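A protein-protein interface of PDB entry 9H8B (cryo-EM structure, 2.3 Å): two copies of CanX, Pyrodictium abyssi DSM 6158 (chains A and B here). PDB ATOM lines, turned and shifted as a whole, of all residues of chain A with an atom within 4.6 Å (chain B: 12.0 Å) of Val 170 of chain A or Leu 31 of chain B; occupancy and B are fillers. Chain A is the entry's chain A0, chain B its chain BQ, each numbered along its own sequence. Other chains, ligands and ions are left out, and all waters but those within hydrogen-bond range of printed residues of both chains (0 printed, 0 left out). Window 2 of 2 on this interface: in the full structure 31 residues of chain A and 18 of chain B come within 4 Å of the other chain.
The side-chain hydroxyl (OG) of Ser 29 of chain B lies within hydrogen-bond range of the side-chain carboxylate (OE1) of Glu 45 of chain A, at 3.3 Å. The backbone NH (N) of Phe 168 of chain A is in hydrogen-bond range of the backbone carbonyl oxygen (O) of Phe 34 of chain B (3.3 Å). The backbone carbonyl oxygen (O) of Leu 31 of chain B is in hydrogen-bond range of the backbone NH (N) of Val 170 of chain A (3.2 Å).
OG of Ser 29 of chain B sits at hydrogen-bond distance from N of Leu 31 of chain B.
Among the printed residues, merely in contact across the chains: Glu 45 of chain A with Leu 31 of chain B, Ile 47 of chain A with Phe 34 of chain B, Phe 168 of chain A with Asn 32 of chain B and Gln 169 of chain A with Leu 31 of chain B.
Leu 31 of chain B touches just these residues of chain A: Glu 45, Gln 169 and Val 170. No residue of chain B comes within 4 Å of Pro 46 of chain A. Printed residues of chain B within 4 Å of Ile 47 of chain A: Phe 34. Leu 85 of chain A touches none of the printed residues of chain B. Of chain B, only Leu 31 (3.5 Å) comes within 4 Å of Gln 169 of chain A. No residue of chain B comes within 4 Å of Ser 172 of chain A. Of the printed residues of chain A, Asn 32 of chain B touches Phe 168 (3.6 Å). Of the printed residues of chain A, Ser 29 of chain B touches Glu 45 (3.3 Å). Printed residues of chain B within 4 Å of Phe 168 of chain A: Asn 32 and Phe 34. Lys 84 of chain A touches none of the printed residues of chain B. The nearest residue of chain A that does not touch Leu 31 of chain B is Pro 46 of chain A (4.04 Å).
Hydrophobic or aromatic side chains of chain A within 4 Å of the printed part of chain B: Phe 168. Hydrophobic or aromatic side chains of chain B within 4 Å of the printed part of chain A: Leu 31 and Phe 34.
No position is printed for both chains. Of the 7 pairs that touch across the chains among the printed residues, none has its exchanged pair printed and touching as well.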
ATOM      1  N   GLU A  45     -10.447 -11.871 -33.901  1.00  0.00           N
ATOM      2  CA  GLU A  45     -10.130 -11.584 -32.512  1.00  0.00           C
ATOM      3  C   GLU A  45      -9.016 -12.503 -32.011  1.00  0.00           C
ATOM      4  O   GLU A  45      -8.834 -13.608 -32.528  1.00  0.00           O
ATOM      5  CB  GLU A  45     -11.373 -11.743 -31.640  1.00  0.00           C
ATOM      6  CG  GLU A  45     -12.383 -10.616 -31.804  1.00  0.00           C
ATOM      7  CD  GLU A  45     -13.625 -10.811 -30.955  1.00  0.00           C
ATOM      8  OE1 GLU A  45     -13.985  -9.876 -30.208  1.00  0.00           O
ATOM      9  OE2 GLU A  45     -14.239 -11.894 -31.034  1.00  0.00           O
ATOM     10  N   PRO A  46      -8.247 -12.057 -31.009  1.00  0.00           N
ATOM     11  CA  PRO A  46      -7.074 -12.843 -30.583  1.00  0.00           C
ATOM     12  C   PRO A  46      -7.396 -14.254 -30.118  1.00  0.00           C
ATOM     13  O   PRO A  46      -6.631 -15.180 -30.413  1.00  0.00           O
ATOM     14  CB  PRO A  46      -6.479 -12.002 -29.442  1.00  0.00           C
ATOM     15  CG  PRO A  46      -7.539 -11.010 -29.072  1.00  0.00           C
ATOM     16  CD  PRO A  46      -8.329 -10.765 -30.309  1.00  0.00           C
ATOM     17  N   ILE A  47      -8.505 -14.455 -29.401  1.00  0.00           N
ATOM     18  CA  ILE A  47      -8.784 -15.736 -28.769  1.00  0.00           C
ATOM     19  C   ILE A  47     -10.197 -16.194 -29.107  1.00  0.00           C
ATOM     20  O   ILE A  47     -11.058 -15.406 -29.506  1.00  0.00           O
ATOM     21  CB  ILE A  47      -8.602 -15.688 -27.234  1.00  0.00           C
ATOM     22  CG1 ILE A  47      -9.695 -14.833 -26.591  1.00  0.00           C
ATOM     23  CG2 ILE A  47      -7.218 -15.170 -26.864  1.00  0.00           C
ATOM     24  CD1 ILE A  47      -9.695 -14.888 -25.080  1.00  0.00           C
ATOM     25  N   LYS A  84      -3.452 -11.769 -21.338  1.00  0.00           N
ATOM     26  CA  LYS A  84      -3.882 -11.378 -20.003  1.00  0.00           C
ATOM     27  C   LYS A  84      -5.404 -11.393 -19.955  1.00  0.00           C
ATOM     28  O   LYS A  84      -6.060 -10.783 -20.808  1.00  0.00           O
ATOM     29  CB  LYS A  84      -3.346  -9.993 -19.635  1.00  0.00           C
ATOM     30  CG  LYS A  84      -2.922  -9.856 -18.182  1.00  0.00           C
ATOM     31  CD  LYS A  84      -2.271  -8.507 -17.918  1.00  0.00           C
ATOM     32  CE  LYS A  84      -3.058  -7.700 -16.899  1.00  0.00           C
ATOM     33  NZ  LYS A  84      -2.614  -6.278 -16.859  1.00  0.00           N
ATOM     34  N   LEU A  85      -5.961 -12.086 -18.966  1.00  0.00           N
ATOM     35  CA  LEU A  85      -7.395 -12.323 -18.898  1.00  0.00           C
ATOM     36  C   LEU A  85      -7.942 -11.915 -17.537  1.00  0.00           C
ATOM     37  O   LEU A  85      -7.227 -11.897 -16.532  1.00  0.00           O
ATOM     38  CB  LEU A  85      -7.730 -13.797 -19.166  1.00  0.00           C
ATOM     39  CG  LEU A  85      -7.492 -14.301 -20.590  1.00  0.00           C
ATOM     40  CD1 LEU A  85      -7.722 -15.801 -20.669  1.00  0.00           C
ATOM     41  CD2 LEU A  85      -8.386 -13.567 -21.576  1.00  0.00           C
ATOM     42  N   PHE A 168     -15.501 -13.825 -19.504  1.00  0.00           N
ATOM     43  CA  PHE A 168     -14.097 -13.606 -19.822  1.00  0.00           C
ATOM     44  C   PHE A 168     -13.933 -12.283 -20.557  1.00  0.00           C
ATOM     45  O   PHE A 168     -14.760 -11.924 -21.401  1.00  0.00           O
ATOM     46  CB  PHE A 168     -13.530 -14.744 -20.682  1.00  0.00           C
ATOM     47  CG  PHE A 168     -13.593 -16.096 -20.026  1.00  0.00           C
ATOM     48  CD1 PHE A 168     -14.771 -16.825 -20.015  1.00  0.00           C
ATOM     49  CD2 PHE A 168     -12.469 -16.638 -19.426  1.00  0.00           C
ATOM     50  CE1 PHE A 168     -14.828 -18.068 -19.414  1.00  0.00           C
ATOM     51  CE2 PHE A 168     -12.520 -17.882 -18.823  1.00  0.00           C
ATOM     52  CZ  PHE A 168     -13.700 -18.596 -18.817  1.00  0.00           C
ATOM     53  N   GLN A 169     -12.863 -11.559 -20.230  1.00  0.00           N
ATOM     54  CA  GLN A 169     -12.536 -10.309 -20.898  1.00  0.00           C
ATOM     55  C   GLN A 169     -11.027 -10.215 -21.076  1.00  0.00           C
ATOM     56  O   GLN A 169     -10.259 -10.528 -20.161  1.00  0.00           O
ATOM     57  CB  GLN A 169     -13.055  -9.093 -20.115  1.00  0.00           C
ATOM     58  CG  GLN A 169     -12.620  -7.752 -20.688  1.00  0.00           C
ATOM     59  CD  GLN A 169     -12.767  -6.615 -19.697  1.00  0.00           C
ATOM     60  OE1 GLN A 169     -12.831  -5.447 -20.079  1.00  0.00           O
ATOM     61  NE2 GLN A 169     -12.819  -6.951 -18.414  1.00  0.00           N
ATOM     62  N   VAL A 170     -10.609  -9.781 -22.261  1.00  0.00           N
ATOM     63  CA  VAL A 170      -9.197  -9.657 -22.610  1.00  0.00           C
ATOM     64  C   VAL A 170      -8.728  -8.252 -22.263  1.00  0.00           C
ATOM     65  O   VAL A 170      -9.347  -7.262 -22.674  1.00  0.00           O
ATOM     66  CB  VAL A 170      -8.963  -9.959 -24.100  1.00  0.00           C
ATOM     67  CG1 VAL A 170      -7.510  -9.700 -24.473  1.00  0.00           C
ATOM     68  CG2 VAL A 170      -9.353 -11.389 -24.417  1.00  0.00           C
ATOM     69  N   LEU A 171      -7.635  -8.163 -21.508  1.00  0.00           N
ATOM     70  CA  LEU A 171      -7.061  -6.879 -21.126  1.00  0.00           C
ATOM     71  C   LEU A 171      -5.852  -6.490 -21.963  1.00  0.00           C
ATOM     72  O   LEU A 171      -5.686  -5.306 -22.276  1.00  0.00           O
ATOM     73  CB  LEU A 171      -6.660  -6.897 -19.648  1.00  0.00           C
ATOM     74  CG  LEU A 171      -7.794  -7.157 -18.654  1.00  0.00           C
ATOM     75  CD1 LEU A 171      -7.238  -7.584 -17.305  1.00  0.00           C
ATOM     76  CD2 LEU A 171      -8.677  -5.928 -18.512  1.00  0.00           C
ATOM     77  N   SER A 172      -5.010  -7.452 -22.336  1.00  0.00           N
ATOM     78  CA  SER A 172      -3.829  -7.171 -23.138  1.00  0.00           C
ATOM     79  C   SER A 172      -3.339  -8.467 -23.765  1.00  0.00           C
ATOM     80  O   SER A 172      -3.399  -9.526 -23.137  1.00  0.00           O
ATOM     81  CB  SER A 172      -2.717  -6.534 -22.298  1.00  0.00           C
ATOM     82  OG  SER A 172      -1.543  -6.342 -23.068  1.00  0.00           O
ATOM     83  N   THR B  27     -13.796  -1.181 -37.177  1.00  0.00           N
ATOM     84  CA  THR B  27     -14.686  -1.541 -36.082  1.00  0.00           C
ATOM     85  C   THR B  27     -13.882  -1.696 -34.800  1.00  0.00           C
ATOM     86  O   THR B  27     -12.823  -2.335 -34.800  1.00  0.00           O
ATOM     87  CB  THR B  27     -15.447  -2.833 -36.389  1.00  0.00           C
ATOM     88  OG1 THR B  27     -15.953  -2.785 -37.729  1.00  0.00           O
ATOM     89  CG2 THR B  27     -16.608  -3.011 -35.422  1.00  0.00           C
ATOM     90  N   GLN B  28     -14.383  -1.113 -33.715  1.00  0.00           N
ATOM     91  CA  GLN B  28     -13.746  -1.188 -32.406  1.00  0.00           C
ATOM     92  C   GLN B  28     -14.498  -2.199 -31.548  1.00  0.00           C
ATOM     93  O   GLN B  28     -15.714  -2.080 -31.366  1.00  0.00           O
ATOM     94  CB  GLN B  28     -13.737   0.186 -31.733  1.00  0.00           C
ATOM     95  CG  GLN B  28     -13.092   0.242 -30.350  1.00  0.00           C
ATOM     96  CD  GLN B  28     -11.677  -0.312 -30.327  1.00  0.00           C
ATOM     97  OE1 GLN B  28     -10.711   0.422 -30.540  1.00  0.00           O
ATOM     98  NE2 GLN B  28     -11.546  -1.601 -30.038  1.00  0.00           N
ATOM     99  N   SER B  29     -13.774  -3.185 -31.021  1.00  0.00           N
ATOM    100  CA  SER B  29     -14.432  -4.245 -30.267  1.00  0.00           C
ATOM    101  C   SER B  29     -14.161  -4.107 -28.773  1.00  0.00           C
ATOM    102  O   SER B  29     -13.061  -3.708 -28.374  1.00  0.00           O
ATOM    103  CB  SER B  29     -13.952  -5.618 -30.741  1.00  0.00           C
ATOM    104  OG  SER B  29     -14.376  -6.643 -29.858  1.00  0.00           O
ATOM    105  N   PRO B  30     -15.147  -4.433 -27.927  1.00  0.00           N
ATOM    106  CA  PRO B  30     -14.918  -4.372 -26.476  1.00  0.00           C
ATOM    107  C   PRO B  30     -14.218  -5.596 -25.910  1.00  0.00           C
ATOM    108  O   PRO B  30     -13.682  -5.513 -24.795  1.00  0.00           O
ATOM    109  CB  PRO B  30     -16.335  -4.236 -25.908  1.00  0.00           C
ATOM    110  CG  PRO B  30     -17.188  -4.962 -26.897  1.00  0.00           C
ATOM    111  CD  PRO B  30     -16.542  -4.781 -28.254  1.00  0.00           C
ATOM    112  N   LEU B  31     -14.215  -6.720 -26.631  1.00  0.00           N
ATOM    113  CA  LEU B  31     -13.459  -7.917 -26.255  1.00  0.00           C
ATOM    114  C   LEU B  31     -13.934  -8.494 -24.919  1.00  0.00           C
ATOM    115  O   LEU B  31     -13.137  -8.805 -24.032  1.00  0.00           O
ATOM    116  CB  LEU B  31     -11.957  -7.623 -26.218  1.00  0.00           C
ATOM    117  CG  LEU B  31     -11.278  -7.300 -27.551  1.00  0.00           C
ATOM    118  CD1 LEU B  31      -9.937  -6.621 -27.315  1.00  0.00           C
ATOM    119  CD2 LEU B  31     -11.107  -8.556 -28.389  1.00  0.00           C
ATOM    120  N   ASN B  32     -15.257  -8.636 -24.776  1.00  0.00           N
ATOM    121  CA  ASN B  32     -15.821  -9.226 -23.566  1.00  0.00           C
ATOM    122  C   ASN B  32     -17.000 -10.147 -23.871  1.00  0.00           C
ATOM    123  O   ASN B  32     -17.830 -10.406 -22.992  1.00  0.00           O
ATOM    124  CB  ASN B  32     -16.239  -8.138 -22.571  1.00  0.00           C
ATOM    125  CG  ASN B  32     -17.174  -7.107 -23.182  1.00  0.00           C
ATOM    126  OD1 ASN B  32     -17.809  -7.348 -24.208  1.00  0.00           O
ATOM    127  ND2 ASN B  32     -17.258  -5.943 -22.548  1.00  0.00           N
ATOM    128  N   SER B  33     -17.092 -10.650 -25.098  1.00  0.00           N
ATOM    129  CA  SER B  33     -18.209 -11.502 -25.511  1.00  0.00           C
ATOM    130  C   SER B  33     -17.840 -12.981 -25.402  1.00  0.00           C
ATOM    131  O   SER B  33     -17.799 -13.717 -26.389  1.00  0.00           O
ATOM    132  CB  SER B  33     -18.648 -11.143 -26.928  1.00  0.00           C
ATOM    133  OG  SER B  33     -19.459  -9.981 -26.932  1.00  0.00           O
ATOM    134  N   PHE B  34     -17.564 -13.418 -24.174  1.00  0.00           N
ATOM    135  CA  PHE B  34     -17.236 -14.811 -23.897  1.00  0.00           C
ATOM    136  C   PHE B  34     -17.935 -15.251 -22.619  1.00  0.00           C
ATOM    137  O   PHE B  34     -17.934 -14.522 -21.623  1.00  0.00           O
ATOM    138  CB  PHE B  34     -15.720 -15.012 -23.774  1.00  0.00           C
ATOM    139  CG  PHE B  34     -14.935 -14.391 -24.895  1.00  0.00           C
ATOM    140  CD1 PHE B  34     -14.820 -15.035 -26.116  1.00  0.00           C
ATOM    141  CD2 PHE B  34     -14.321 -13.161 -24.732  1.00  0.00           C
ATOM    142  CE1 PHE B  34     -14.101 -14.467 -27.150  1.00  0.00           C
ATOM    143  CE2 PHE B  34     -13.602 -12.586 -25.763  1.00  0.00           C
ATOM    144  CZ  PHE B  34     -13.491 -13.241 -26.974  1.00  0.00           C
ATOM    145  N   TYR B  35     -18.531 -16.443 -22.650  1.00  0.00           N
ATOM    146  CA  TYR B  35     -19.304 -16.930 -21.516  1.00  0.00           C
ATOM    147  C   TYR B  35     -19.173 -18.442 -21.397  1.00  0.00           C
ATOM    148  O   TYR B  35     -18.829 -19.138 -22.356  1.00  0.00           O
ATOM    149  CB  TYR B  35     -20.784 -16.542 -21.635  1.00  0.00           C
ATOM    150  CG  TYR B  35     -21.066 -15.079 -21.376  1.00  0.00           C
ATOM    151  CD1 TYR B  35     -21.351 -14.626 -20.094  1.00  0.00           C
ATOM    152  CD2 TYR B  35     -21.061 -14.154 -22.411  1.00  0.00           C
ATOM    153  CE1 TYR B  35     -21.612 -13.292 -19.849  1.00  0.00           C
ATOM    154  CE2 TYR B  35     -21.320 -12.816 -22.176  1.00  0.00           C
ATOM    155  CZ  TYR B  35     -21.596 -12.392 -20.893  1.00  0.00           C
ATOM    156  OH  TYR B  35     -21.858 -11.062 -20.653  1.00  0.00           O
